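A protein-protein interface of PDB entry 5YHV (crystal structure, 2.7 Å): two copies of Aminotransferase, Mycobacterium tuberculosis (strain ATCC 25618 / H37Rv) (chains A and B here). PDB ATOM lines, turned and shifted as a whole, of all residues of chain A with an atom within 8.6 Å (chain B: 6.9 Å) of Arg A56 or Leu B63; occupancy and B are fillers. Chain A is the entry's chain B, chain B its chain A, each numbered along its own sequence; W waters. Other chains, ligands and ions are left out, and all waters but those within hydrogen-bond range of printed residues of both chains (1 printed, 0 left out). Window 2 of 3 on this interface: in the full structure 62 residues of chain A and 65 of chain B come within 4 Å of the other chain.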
ATOM      1  N   SER A  48     -11.607  28.412 -24.312  1.00  0.00           N
ATOM      2  CA  SER A  48     -11.553  28.288 -22.857  1.00  0.00           C
ATOM      3  C   SER A  48     -12.302  27.041 -22.382  1.00  0.00           C
ATOM      4  O   SER A  48     -12.018  26.513 -21.304  1.00  0.00           O
ATOM      5  CB  SER A  48     -12.098  29.546 -22.183  1.00  0.00           C
ATOM      6  OG  SER A  48     -13.418  29.820 -22.616  1.00  0.00           O
ATOM      7  N   ALA A  49     -13.254  26.582 -23.194  1.00  0.00           N
ATOM      8  CA  ALA A  49     -13.976  25.331 -22.954  1.00  0.00           C
ATOM      9  C   ALA A  49     -13.126  24.111 -23.310  1.00  0.00           C
ATOM     10  O   ALA A  49     -12.224  24.195 -24.149  1.00  0.00           O
ATOM     11  CB  ALA A  49     -15.278  25.313 -23.737  1.00  0.00           C
ATOM     12  N   GLY A  50     -13.418  22.988 -22.658  1.00  0.00           N
ATOM     13  CA  GLY A  50     -12.801  21.706 -22.981  1.00  0.00           C
ATOM     14  C   GLY A  50     -13.658  20.888 -23.931  1.00  0.00           C
ATOM     15  O   GLY A  50     -14.617  21.399 -24.519  1.00  0.00           O
ATOM     16  N   ALA A  51     -13.308  19.608 -24.065  1.00  0.00           N
ATOM     17  CA  ALA A  51     -14.021  18.656 -24.921  1.00  0.00           C
ATOM     18  C   ALA A  51     -15.484  18.499 -24.489  1.00  0.00           C
ATOM     19  O   ALA A  51     -15.782  18.629 -23.301  1.00  0.00           O
ATOM     20  CB  ALA A  51     -13.316  17.307 -24.890  1.00  0.00           C
ATOM     21  N   PRO A  52     -16.405  18.231 -25.448  1.00  0.00           N
ATOM     22  CA  PRO A  52     -17.798  18.012 -25.062  1.00  0.00           C
ATOM     23  C   PRO A  52     -17.946  16.754 -24.210  1.00  0.00           C
ATOM     24  O   PRO A  52     -17.145  15.820 -24.341  1.00  0.00           O
ATOM     25  CB  PRO A  52     -18.517  17.828 -26.402  1.00  0.00           C
ATOM     26  CG  PRO A  52     -17.601  18.396 -27.425  1.00  0.00           C
ATOM     27  CD  PRO A  52     -16.235  18.091 -26.909  1.00  0.00           C
ATOM     28  N   GLU A  53     -18.962  16.740 -23.351  1.00  0.00           N
ATOM     29  CA  GLU A  53     -19.178  15.635 -22.411  1.00  0.00           C
ATOM     30  C   GLU A  53     -19.317  14.231 -23.038  1.00  0.00           C
ATOM     31  O   GLU A  53     -18.808  13.271 -22.448  1.00  0.00           O
ATOM     32  CB  GLU A  53     -20.326  15.931 -21.429  1.00  0.00           C
ATOM     33  CG  GLU A  53     -20.056  17.068 -20.444  1.00  0.00           C
ATOM     34  CD  GLU A  53     -18.835  16.850 -19.551  1.00  0.00           C
ATOM     35  OE1 GLU A  53     -18.117  17.837 -19.284  1.00  0.00           O
ATOM     36  OE2 GLU A  53     -18.582  15.710 -19.103  1.00  0.00           O
ATOM     37  N   PRO A  54     -19.978  14.100 -24.222  1.00  0.00           N
ATOM     38  CA  PRO A  54     -19.975  12.775 -24.872  1.00  0.00           C
ATOM     39  C   PRO A  54     -18.590  12.267 -25.269  1.00  0.00           C
ATOM     40  O   PRO A  54     -18.345  11.055 -25.210  1.00  0.00           O
ATOM     41  CB  PRO A  54     -20.840  12.990 -26.113  1.00  0.00           C
ATOM     42  CG  PRO A  54     -21.775  14.077 -25.712  1.00  0.00           C
ATOM     43  CD  PRO A  54     -20.932  15.008 -24.894  1.00  0.00           C
ATOM     44  N   VAL A  55     -17.703  13.187 -25.656  1.00  0.00           N
ATOM     45  CA  VAL A  55     -16.313  12.861 -25.992  1.00  0.00           C
ATOM     46  C   VAL A  55     -15.578  12.383 -24.734  1.00  0.00           C
ATOM     47  O   VAL A  55     -14.913  11.344 -24.757  1.00  0.00           O
ATOM     48  CB  VAL A  55     -15.589  14.055 -26.678  1.00  0.00           C
ATOM     49  CG1 VAL A  55     -14.089  13.817 -26.809  1.00  0.00           C
ATOM     50  CG2 VAL A  55     -16.194  14.333 -28.046  1.00  0.00           C
ATOM     51  N   ARG A  56     -15.733  13.129 -23.641  1.00  0.00           N
ATOM     52  CA  ARG A  56     -15.120  12.777 -22.354  1.00  0.00           C
ATOM     53  C   ARG A  56     -15.634  11.440 -21.814  1.00  0.00           C
ATOM     54  O   ARG A  56     -14.851  10.645 -21.283  1.00  0.00           O
ATOM     55  CB  ARG A  56     -15.334  13.883 -21.320  1.00  0.00           C
ATOM     56  CG  ARG A  56     -14.754  15.233 -21.711  1.00  0.00           C
ATOM     57  CD  ARG A  56     -14.759  16.172 -20.526  1.00  0.00           C
ATOM     58  NE  ARG A  56     -14.749  17.569 -20.940  1.00  0.00           N
ATOM     59  CZ  ARG A  56     -14.607  18.608 -20.119  1.00  0.00           C
ATOM     60  NH1 ARG A  56     -14.451  18.428 -18.813  1.00  0.00           N
ATOM     61  NH2 ARG A  56     -14.615  19.842 -20.612  1.00  0.00           N
ATOM     62  N   ALA A  57     -16.940  11.202 -21.968  1.00  0.00           N
ATOM     63  CA  ALA A  57     -17.575   9.950 -21.557  1.00  0.00           C
ATOM     64  C   ALA A  57     -17.045   8.746 -22.333  1.00  0.00           C
ATOM     65  O   ALA A  57     -16.808   7.684 -21.747  1.00  0.00           O
ATOM     66  CB  ALA A  57     -19.078  10.044 -21.704  1.00  0.00           C
ATOM     67  N   ALA A  58     -16.858   8.927 -23.642  1.00  0.00           N
ATOM     68  CA  ALA A  58     -16.321   7.881 -24.509  1.00  0.00           C
ATOM     69  C   ALA A  58     -14.880   7.525 -24.136  1.00  0.00           C
ATOM     70  O   ALA A  58     -14.515   6.349 -24.151  1.00  0.00           O
ATOM     71  CB  ALA A  58     -16.426   8.290 -25.971  1.00  0.00           C
ATOM     72  N   ALA A  59     -14.083   8.538 -23.788  1.00  0.00           N
ATOM     73  CA  ALA A  59     -12.706   8.336 -23.333  1.00  0.00           C
ATOM     74  C   ALA A  59     -12.656   7.606 -21.987  1.00  0.00           C
ATOM     75  O   ALA A  59     -11.859   6.684 -21.805  1.00  0.00           O
ATOM     76  CB  ALA A  59     -11.969   9.665 -23.250  1.00  0.00           C
ATOM     77  N   ALA A  60     -13.523   8.019 -21.062  1.00  0.00           N
ATOM     78  CA  ALA A  60     -13.640   7.406 -19.738  1.00  0.00           C
ATOM     79  C   ALA A  60     -13.998   5.920 -19.812  1.00  0.00           C
ATOM     80  O   ALA A  60     -13.433   5.105 -19.072  1.00  0.00           O
ATOM     81  CB  ALA A  60     -14.653   8.164 -18.894  1.00  0.00           C
ATOM     82  N   ALA A  61     -14.921   5.583 -20.717  1.00  0.00           N
ATOM     83  CA  ALA A  61     -15.317   4.198 -20.981  1.00  0.00           C
ATOM     84  C   ALA A  61     -14.198   3.393 -21.659  1.00  0.00           C
ATOM     85  O   ALA A  61     -13.965   2.227 -21.304  1.00  0.00           O
ATOM     86  CB  ALA A  61     -16.587   4.162 -21.813  1.00  0.00           C
ATOM     87  N   ALA A  62     -13.506   4.028 -22.610  1.00  0.00           N
ATOM     88  CA  ALA A  62     -12.408   3.401 -23.352  1.00  0.00           C
ATOM     89  C   ALA A  62     -11.224   3.012 -22.463  1.00  0.00           C
ATOM     90  O   ALA A  62     -10.561   2.007 -22.724  1.00  0.00           O
ATOM     91  CB  ALA A  62     -11.945   4.295 -24.491  1.00  0.00           C
ATOM     92  N   LEU A  63     -10.976   3.802 -21.415  1.00  0.00           N
ATOM     93  CA  LEU A  63      -9.936   3.500 -20.424  1.00  0.00           C
ATOM     94  C   LEU A  63     -10.171   2.172 -19.687  1.00  0.00           C
ATOM     95  O   LEU A  63      -9.222   1.542 -19.211  1.00  0.00           O
ATOM     96  CB  LEU A  63      -9.790   4.652 -19.425  1.00  0.00           C
ATOM     97  CG  LEU A  63      -9.182   5.966 -19.934  1.00  0.00           C
ATOM     98  CD1 LEU A  63      -9.490   7.115 -18.989  1.00  0.00           C
ATOM     99  CD2 LEU A  63      -7.686   5.836 -20.119  1.00  0.00           C
ATOM    100  N   TYR A 242     -14.589  21.703 -31.909  1.00  0.00           N
ATOM    101  CA  TYR A 242     -14.907  20.709 -30.888  1.00  0.00           C
ATOM    102  C   TYR A 242     -14.119  20.871 -29.591  1.00  0.00           C
ATOM    103  O   TYR A 242     -14.231  20.030 -28.690  1.00  0.00           O
ATOM    104  CB  TYR A 242     -14.766  19.292 -31.448  1.00  0.00           C
ATOM    105  CG  TYR A 242     -15.913  18.899 -32.339  1.00  0.00           C
ATOM    106  CD1 TYR A 242     -17.208  18.783 -31.824  1.00  0.00           C
ATOM    107  CD2 TYR A 242     -15.712  18.644 -33.702  1.00  0.00           C
ATOM    108  CE1 TYR A 242     -18.273  18.435 -32.638  1.00  0.00           C
ATOM    109  CE2 TYR A 242     -16.771  18.289 -34.527  1.00  0.00           C
ATOM    110  CZ  TYR A 242     -18.049  18.185 -33.988  1.00  0.00           C
ATOM    111  OH  TYR A 242     -19.108  17.832 -34.792  1.00  0.00           O
ATOM    112  N   ALA A 243     -13.334  21.949 -29.504  1.00  0.00           N
ATOM    113  CA  ALA A 243     -12.551  22.316 -28.308  1.00  0.00           C
ATOM    114  C   ALA A 243     -11.687  21.187 -27.705  1.00  0.00           C
ATOM    115  O   ALA A 243     -11.462  21.131 -26.490  1.00  0.00           O
ATOM    116  CB  ALA A 243     -13.453  22.965 -27.255  1.00  0.00           C
ATOM    117  N   MET A 244     -11.193  20.304 -28.572  1.00  0.00           N
ATOM    118  CA  MET A 244     -10.362  19.164 -28.167  1.00  0.00           C
ATOM    119  C   MET A 244      -8.880  19.461 -28.382  1.00  0.00           C
ATOM    120  O   MET A 244      -8.103  18.607 -28.807  1.00  0.00           O
ATOM    121  CB  MET A 244     -10.785  17.906 -28.917  1.00  0.00           C
ATOM    122  CG  MET A 244     -12.105  17.321 -28.464  1.00  0.00           C
ATOM    123  SD  MET A 244     -12.595  15.961 -29.526  1.00  0.00           S
ATOM    124  CE  MET A 244     -11.324  14.742 -29.184  1.00  0.00           C
ATOM    125  N   TRP A 247      -6.060  17.279 -27.017  1.00  0.00           N
ATOM    126  CA  TRP A 247      -6.238  15.883 -27.429  1.00  0.00           C
ATOM    127  C   TRP A 247      -5.376  15.533 -28.641  1.00  0.00           C
ATOM    128  O   TRP A 247      -5.187  14.361 -28.944  1.00  0.00           O
ATOM    129  CB  TRP A 247      -7.708  15.588 -27.726  1.00  0.00           C
ATOM    130  CG  TRP A 247      -8.634  15.723 -26.540  1.00  0.00           C
ATOM    131  CD1 TRP A 247      -8.961  16.875 -25.876  1.00  0.00           C
ATOM    132  CD2 TRP A 247      -9.363  14.671 -25.896  1.00  0.00           C
ATOM    133  NE1 TRP A 247      -9.832  16.604 -24.850  1.00  0.00           N
ATOM    134  CE2 TRP A 247     -10.100  15.261 -24.839  1.00  0.00           C
ATOM    135  CE3 TRP A 247      -9.464  13.289 -26.103  1.00  0.00           C
ATOM    136  CZ2 TRP A 247     -10.934  14.514 -23.995  1.00  0.00           C
ATOM    137  CZ3 TRP A 247     -10.290  12.541 -25.260  1.00  0.00           C
ATOM    138  CH2 TRP A 247     -11.015  13.158 -24.221  1.00  0.00           C
ATOM    139  N   LEU A 276      -6.772   7.057 -27.723  1.00  0.00           N
ATOM    140  CA  LEU A 276      -7.833   7.488 -26.811  1.00  0.00           C
ATOM    141  C   LEU A 276      -8.601   8.681 -27.388  1.00  0.00           C
ATOM    142  O   LEU A 276      -9.826   8.736 -27.285  1.00  0.00           O
ATOM    143  CB  LEU A 276      -7.274   7.796 -25.411  1.00  0.00           C
ATOM    144  CG  LEU A 276      -8.243   8.079 -24.255  1.00  0.00           C
ATOM    145  CD1 LEU A 276      -9.219   6.932 -24.006  1.00  0.00           C
ATOM    146  CD2 LEU A 276      -7.455   8.373 -22.989  1.00  0.00           C
ATOM    147  N   ILE A 279     -10.883   7.222 -30.379  1.00  0.00           N
ATOM    148  CA  ILE A 279     -12.069   6.519 -29.874  1.00  0.00           C
ATOM    149  C   ILE A 279     -13.093   7.528 -29.338  1.00  0.00           C
ATOM    150  O   ILE A 279     -14.285   7.436 -29.651  1.00  0.00           O
ATOM    151  CB  ILE A 279     -11.699   5.443 -28.814  1.00  0.00           C
ATOM    152  CG1 ILE A 279     -10.867   4.323 -29.453  1.00  0.00           C
ATOM    153  CG2 ILE A 279     -12.950   4.855 -28.162  1.00  0.00           C
ATOM    154  CD1 ILE A 279     -10.043   3.488 -28.487  1.00  0.00           C
ATOM    155  N   ALA A 280     -12.605   8.499 -28.569  1.00  0.00           N
ATOM    156  CA  ALA A 280     -13.436   9.543 -27.979  1.00  0.00           C
ATOM    157  C   ALA A 280     -14.083  10.470 -29.009  1.00  0.00           C
ATOM    158  O   ALA A 280     -15.235  10.882 -28.830  1.00  0.00           O
ATOM    159  CB  ALA A 280     -12.629  10.349 -26.977  1.00  0.00           C
ATOM    160  N   ALA A 281     -13.349  10.782 -30.081  1.00  0.00           N
ATOM    161  CA  ALA A 281     -13.811  11.747 -31.090  1.00  0.00           C
ATOM    162  C   ALA A 281     -14.976  11.268 -31.962  1.00  0.00           C
ATOM    163  O   ALA A 281     -15.660  12.088 -32.577  1.00  0.00           O
ATOM    164  CB  ALA A 281     -12.656  12.221 -31.952  1.00  0.00           C
ATOM    165  N   SER A 283     -17.661  10.177 -30.725  1.00  0.00           N
ATOM    166  CA  SER A 283     -18.778  10.798 -30.004  1.00  0.00           C
ATOM    167  C   SER A 283     -18.915  12.323 -30.180  1.00  0.00           C
ATOM    168  O   SER A 283     -19.855  12.924 -29.645  1.00  0.00           O
ATOM    169  CB  SER A 283     -18.703  10.436 -28.521  1.00  0.00           C
ATOM    170  OG  SER A 283     -18.974   9.063 -28.337  1.00  0.00           O
ATOM    171  N   ALA A 284     -17.993  12.949 -30.920  1.00  0.00           N
ATOM    172  CA  ALA A 284     -18.115  14.375 -31.264  1.00  0.00           C
ATOM    173  C   ALA A 284     -19.251  14.626 -32.254  1.00  0.00           C
ATOM    174  O   ALA A 284     -19.802  15.731 -32.315  1.00  0.00           O
ATOM    175  CB  ALA A 284     -16.804  14.925 -31.809  1.00  0.00           C
ATOM    176  N   ALA A 289     -23.039  16.571 -28.375  1.00  0.00           N
ATOM    177  CA  ALA A 289     -21.728  17.199 -28.559  1.00  0.00           C
ATOM    178  C   ALA A 289     -21.801  18.428 -29.466  1.00  0.00           C
ATOM    179  O   ALA A 289     -21.176  19.457 -29.183  1.00  0.00           O
ATOM    180  CB  ALA A 289     -20.722  16.193 -29.092  1.00  0.00           C
ATOM    181  N   GLU A 292     -23.319  21.373 -27.598  1.00  0.00           N
ATOM    182  CA  GLU A 292     -22.311  21.965 -26.717  1.00  0.00           C
ATOM    183  C   GLU A 292     -21.302  22.812 -27.495  1.00  0.00           C
ATOM    184  O   GLU A 292     -20.890  23.879 -27.026  1.00  0.00           O
ATOM    185  CB  GLU A 292     -21.590  20.880 -25.915  1.00  0.00           C
ATOM    186  CG  GLU A 292     -22.443  20.238 -24.828  1.00  0.00           C
ATOM    187  CD  GLU A 292     -21.719  19.139 -24.067  1.00  0.00           C
ATOM    188  OE1 GLU A 292     -22.334  18.081 -23.821  1.00  0.00           O
ATOM    189  OE2 GLU A 292     -20.537  19.323 -23.706  1.00  0.00           O
ATOM    190  N   ASN A 296     -20.900  26.955 -27.337  1.00  0.00           N
ATOM    191  CA  ASN A 296     -19.653  27.729 -27.262  1.00  0.00           C
ATOM    192  C   ASN A 296     -19.647  28.883 -28.266  1.00  0.00           C
ATOM    193  O   ASN A 296     -19.276  30.007 -27.917  1.00  0.00           O
ATOM    194  CB  ASN A 296     -18.421  26.832 -27.480  1.00  0.00           C
ATOM    195  CG  ASN A 296     -18.173  25.870 -26.327  1.00  0.00           C
ATOM    196  OD1 ASN A 296     -18.358  26.209 -25.152  1.00  0.00           O
ATOM    197  ND2 ASN A 296     -17.733  24.666 -26.657  1.00  0.00           N
ATOM    198  N   ARG B  56      -4.210   5.213 -15.820  1.00  0.00           N
ATOM    199  CA  ARG B  56      -5.610   5.243 -16.260  1.00  0.00           C
ATOM    200  C   ARG B  56      -6.504   6.033 -15.301  1.00  0.00           C
ATOM    201  O   ARG B  56      -7.379   6.788 -15.744  1.00  0.00           O
ATOM    202  CB  ARG B  56      -6.160   3.829 -16.452  1.00  0.00           C
ATOM    203  CG  ARG B  56      -5.409   2.992 -17.472  1.00  0.00           C
ATOM    204  CD  ARG B  56      -6.181   1.738 -17.802  1.00  0.00           C
ATOM    205  NE  ARG B  56      -5.310   0.676 -18.298  1.00  0.00           N
ATOM    206  CZ  ARG B  56      -5.730  -0.458 -18.857  1.00  0.00           C
ATOM    207  NH1 ARG B  56      -7.027  -0.697 -19.020  1.00  0.00           N
ATOM    208  NH2 ARG B  56      -4.847  -1.362 -19.260  1.00  0.00           N
ATOM    209  N   ALA B  58      -5.506   8.485 -13.264  1.00  0.00           N
ATOM    210  CA  ALA B  58      -5.131   9.893 -13.395  1.00  0.00           C
ATOM    211  C   ALA B  58      -5.793  10.541 -14.611  1.00  0.00           C
ATOM    212  O   ALA B  58      -6.230  11.687 -14.531  1.00  0.00           O
ATOM    213  CB  ALA B  58      -3.621  10.045 -13.449  1.00  0.00           C
ATOM    214  N   ALA B  59      -5.881   9.799 -15.717  1.00  0.00           N
ATOM    215  CA  ALA B  59      -6.562  10.261 -16.928  1.00  0.00           C
ATOM    216  C   ALA B  59      -8.068  10.417 -16.704  1.00  0.00           C
ATOM    217  O   ALA B  59      -8.661  11.421 -17.113  1.00  0.00           O
ATOM    218  CB  ALA B  59      -6.283   9.324 -18.091  1.00  0.00           C
ATOM    219  N   ALA B  60      -8.667   9.427 -16.038  1.00  0.00           N
ATOM    220  CA  ALA B  60     -10.094   9.432 -15.702  1.00  0.00           C
ATOM    221  C   ALA B  60     -10.481  10.633 -14.832  1.00  0.00           C
ATOM    222  O   ALA B  60     -11.526  11.256 -15.061  1.00  0.00           O
ATOM    223  CB  ALA B  60     -10.478   8.127 -15.021  1.00  0.00           C
ATOM    224  N   ALA B  61      -9.627  10.950 -13.854  1.00  0.00           N
ATOM    225  CA  ALA B  61      -9.800  12.116 -12.987  1.00  0.00           C
ATOM    226  C   ALA B  61      -9.598  13.436 -13.740  1.00  0.00           C
ATOM    227  O   ALA B  61     -10.352  14.394 -13.529  1.00  0.00           O
ATOM    228  CB  ALA B  61      -8.862  12.029 -11.793  1.00  0.00           C
ATOM    229  N   ALA B  62      -8.594  13.468 -14.622  1.00  0.00           N
ATOM    230  CA  ALA B  62      -8.267  14.658 -15.419  1.00  0.00           C
ATOM    231  C   ALA B  62      -9.388  15.065 -16.374  1.00  0.00           C
ATOM    232  O   ALA B  62      -9.585  16.257 -16.625  1.00  0.00           O
ATOM    233  CB  ALA B  62      -6.969  14.459 -16.178  1.00  0.00           C
ATOM    234  N   LEU B  63     -10.128  14.075 -16.886  1.00  0.00           N
ATOM    235  CA  LEU B  63     -11.297  14.321 -17.741  1.00  0.00           C
ATOM    236  C   LEU B  63     -12.403  15.121 -17.032  1.00  0.00           C
ATOM    237  O   LEU B  63     -13.196  15.807 -17.678  1.00  0.00           O
ATOM    238  CB  LEU B  63     -11.851  13.006 -18.292  1.00  0.00           C
ATOM    239  CG  LEU B  63     -11.014  12.257 -19.335  1.00  0.00           C
ATOM    240  CD1 LEU B  63     -11.461  10.808 -19.463  1.00  0.00           C
ATOM    241  CD2 LEU B  63     -11.073  12.943 -20.687  1.00  0.00           C
ATOM    242  N   HIS B  64     -12.433  15.025 -15.704  1.00  0.00           N
ATOM    243  CA  HIS B  64     -13.356  15.774 -14.866  1.00  0.00           C
ATOM    244  C   HIS B  64     -12.757  17.094 -14.363  1.00  0.00           C
ATOM    245  O   HIS B  64     -13.451  18.119 -14.332  1.00  0.00           O
ATOM    246  CB  HIS B  64     -13.832  14.910 -13.690  1.00  0.00           C
ATOM    247  CG  HIS B  64     -14.860  13.882 -14.067  1.00  0.00           C
ATOM    248  ND1 HIS B  64     -16.156  14.213 -14.397  1.00  0.00           N
ATOM    249  CD2 HIS B  64     -14.784  12.531 -14.158  1.00  0.00           C
ATOM    250  CE1 HIS B  64     -16.834  13.114 -14.676  1.00  0.00           C
ATOM    251  NE2 HIS B  64     -16.022  12.081 -14.549  1.00  0.00           N
ATOM    252  N   LEU B  65     -11.474  17.073 -14.001  1.00  0.00           N
ATOM    253  CA  LEU B  65     -10.826  18.212 -13.338  1.00  0.00           C
ATOM    254  C   LEU B  65     -10.094  19.203 -14.243  1.00  0.00           C
ATOM    255  O   LEU B  65      -9.886  20.356 -13.855  1.00  0.00           O
ATOM    256  CB  LEU B  65      -9.879  17.720 -12.233  1.00  0.00           C
ATOM    257  CG  LEU B  65     -10.493  17.108 -10.972  1.00  0.00           C
ATOM    258  CD1 LEU B  65      -9.405  16.519 -10.091  1.00  0.00           C
ATOM    259  CD2 LEU B  65     -11.326  18.112 -10.191  1.00  0.00           C
ATOM    260  N   ASN B  66      -9.701  18.756 -15.434  1.00  0.00           N
ATOM    261  CA  ASN B  66      -8.869  19.567 -16.323  1.00  0.00           C
ATOM    262  C   ASN B  66      -9.550  19.859 -17.659  1.00  0.00           C
ATOM    263  O   ASN B  66     -10.193  18.990 -18.249  1.00  0.00           O
ATOM    264  CB  ASN B  66      -7.510  18.893 -16.537  1.00  0.00           C
ATOM    265  CG  ASN B  66      -6.437  19.863 -16.986  1.00  0.00           C
ATOM    266  OD1 ASN B  66      -6.434  20.334 -18.129  1.00  0.00           O
ATOM    267  ND2 ASN B  66      -5.502  20.155 -16.091  1.00  0.00           N
ATOM    268  N   GLN B  67      -9.387  21.101 -18.114  1.00  0.00           N
ATOM    269  CA  GLN B  67      -9.889  21.598 -19.404  1.00  0.00           C
ATOM    270  C   GLN B  67      -9.278  20.834 -20.582  1.00  0.00           C
ATOM    271  O   GLN B  67      -9.927  20.657 -21.619  1.00  0.00           O
ATOM    272  CB  GLN B  67      -9.571  23.097 -19.525  1.00  0.00           C
ATOM    273  CG  GLN B  67     -10.111  23.799 -20.766  1.00  0.00           C
ATOM    274  CD  GLN B  67      -9.175  24.877 -21.318  1.00  0.00           C
ATOM    275  OE1 GLN B  67      -9.000  24.988 -22.536  1.00  0.00           O
ATOM    276  NE2 GLN B  67      -8.566  25.670 -20.431  1.00  0.00           N
ATOM    277  N   LEU B  68      -8.038  20.377 -20.397  1.00  0.00           N
ATOM    278  CA  LEU B  68      -7.230  19.721 -21.429  1.00  0.00           C
ATOM    279  C   LEU B  68      -7.001  20.626 -22.642  1.00  0.00           C
ATOM    280  O   LEU B  68      -7.173  20.209 -23.795  1.00  0.00           O
ATOM    281  CB  LEU B  68      -7.797  18.342 -21.827  1.00  0.00           C
ATOM    282  CG  LEU B  68      -8.047  17.275 -20.757  1.00  0.00           C
ATOM    283  CD1 LEU B  68      -8.644  16.043 -21.416  1.00  0.00           C
ATOM    284  CD2 LEU B  68      -6.786  16.909 -19.973  1.00  0.00           C
ATOM    285  N   LEU B 276      -3.727  14.991 -22.005  1.00  0.00           N
ATOM    286  CA  LEU B 276      -4.284  13.921 -21.175  1.00  0.00           C
ATOM    287  C   LEU B 276      -3.231  12.842 -20.889  1.00  0.00           C
ATOM    288  O   LEU B 276      -3.140  12.350 -19.764  1.00  0.00           O
ATOM    289  CB  LEU B 276      -5.555  13.327 -21.800  1.00  0.00           C
ATOM    290  CG  LEU B 276      -6.396  12.329 -20.984  1.00  0.00           C
ATOM    291  CD1 LEU B 276      -6.889  12.905 -19.665  1.00  0.00           C
ATOM    292  CD2 LEU B 276      -7.572  11.825 -21.795  1.00  0.00           C
HETATM  293  O   HOH W   1     -16.408  16.932 -17.162  1.00  0.00           O
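Arg A56 touches one residue of chain B.
Printed residues of chain A within 4 Å of Leu B63: Arg A56 (3.1 Å), Ala A59 (3.99 Å), Ala A60 (3.8 Å) and Trp A247 (3.5 Å).
No residue of chain A comes within 4 Å of Ala B62.
Printed residues of chain B within 4 Å of Ala A59: Leu B63 (3.99 Å).
Of the printed residues of chain B, Gly A50 touches Gln B67.
Printed residues of chain A within 4 Å of Gln B67: Ser A48 (3.3 Å), Ala A49 (3.7 Å) and Gly A50 (3.3 Å).
Printed residues of chain B within 4 Å of Ala A49: Gln B67 (3.7 Å).
Ala A51 touches none of the printed residues of chain B.
The nearest printed residue of chain A that does not touch Leu B63 is Leu A63 (4.2 Å).
Arg A56 touches Leu B63, and with the chains exchanged Leu A63 touches Arg B56.
Ala A59 touches Leu B63, and with the chains exchanged Leu A63 touches Ala B59.
Ala A60 touches Leu B63, and with the chains exchanged Leu A63 touches Ala B60.
Leu B276 touches its own counterpart, Leu A276.
Positions printed for both chains: 56, 58, 59, 60, 61, 62, 63 and 276.
Of the 12 pairs that touch across the chains among the printed residues, 7 have their exchanged pair printed and touching as well.
Among the printed residues, pairs that only touch across the chains: Ser A48 with Gln B67 (3.3 Å), Ala A49 with Gln B67 (3.7 Å), Gly A50 with Gln B67 (3.3 Å), Ala A59 with Leu B63 (3.99 Å), Ala A60 with Leu B63 (3.8 Å), Leu A63 with Ala B59 (3.996 Å), Leu A63 with Ala B60 (3.8 Å), Trp A247 with Leu B63 (3.5 Å), Trp A247 with Leu B68 (3.7 Å) and Leu A276 with Leu B276 (3.7 Å).
Water W1 lies within hydrogen-bond range of OE1 of Glu A53 (2.9 Å), NH1 of Arg A56 (3.0 Å) and O of Leu B63 (3.4 Å).
The backbone carbonyl oxygen (O) of Leu A63 is in hydrogen-bond range of the guanidinium group (NH1) of Arg B56 (3.1 Å).
O of Leu B63 lies within hydrogen-bond range of NH1 of Arg A56, at 3.1 Å.
The side-chain amide oxygen of Asn B66 is in hydrogen-bond range of the backbone NH of Leu B68 (2.8 Å).
The guanidinium group (NE) of Arg A56 lies within hydrogen-bond range of the backbone carbonyl oxygen (O) of Ala A51 (2.8 Å).
OE1 of Glu A53 is in salt-bridge range of NH1 of Arg A56, at 3.7 Å.
Printed residues of chain B that touch a printed residue of chain A: Arg B56, Ala B59, Ala B60, Leu B63, Gln B67, Leu B68 and Leu B276.
Hydrophobic or aromatic side chains of chain A that line the printed part of chain B: Ala A59, Leu A63, Trp A247 and Leu A276.
Along chain A the printed residues that touch a printed residue of chain B span positions 48 to 276.
Among the printed residues, 12 pairs touch across the chains.
Among the printed residues, no Asp or Glu carboxylate lies within 4 Å of a Lys or Arg side-chain nitrogen of the other chain.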
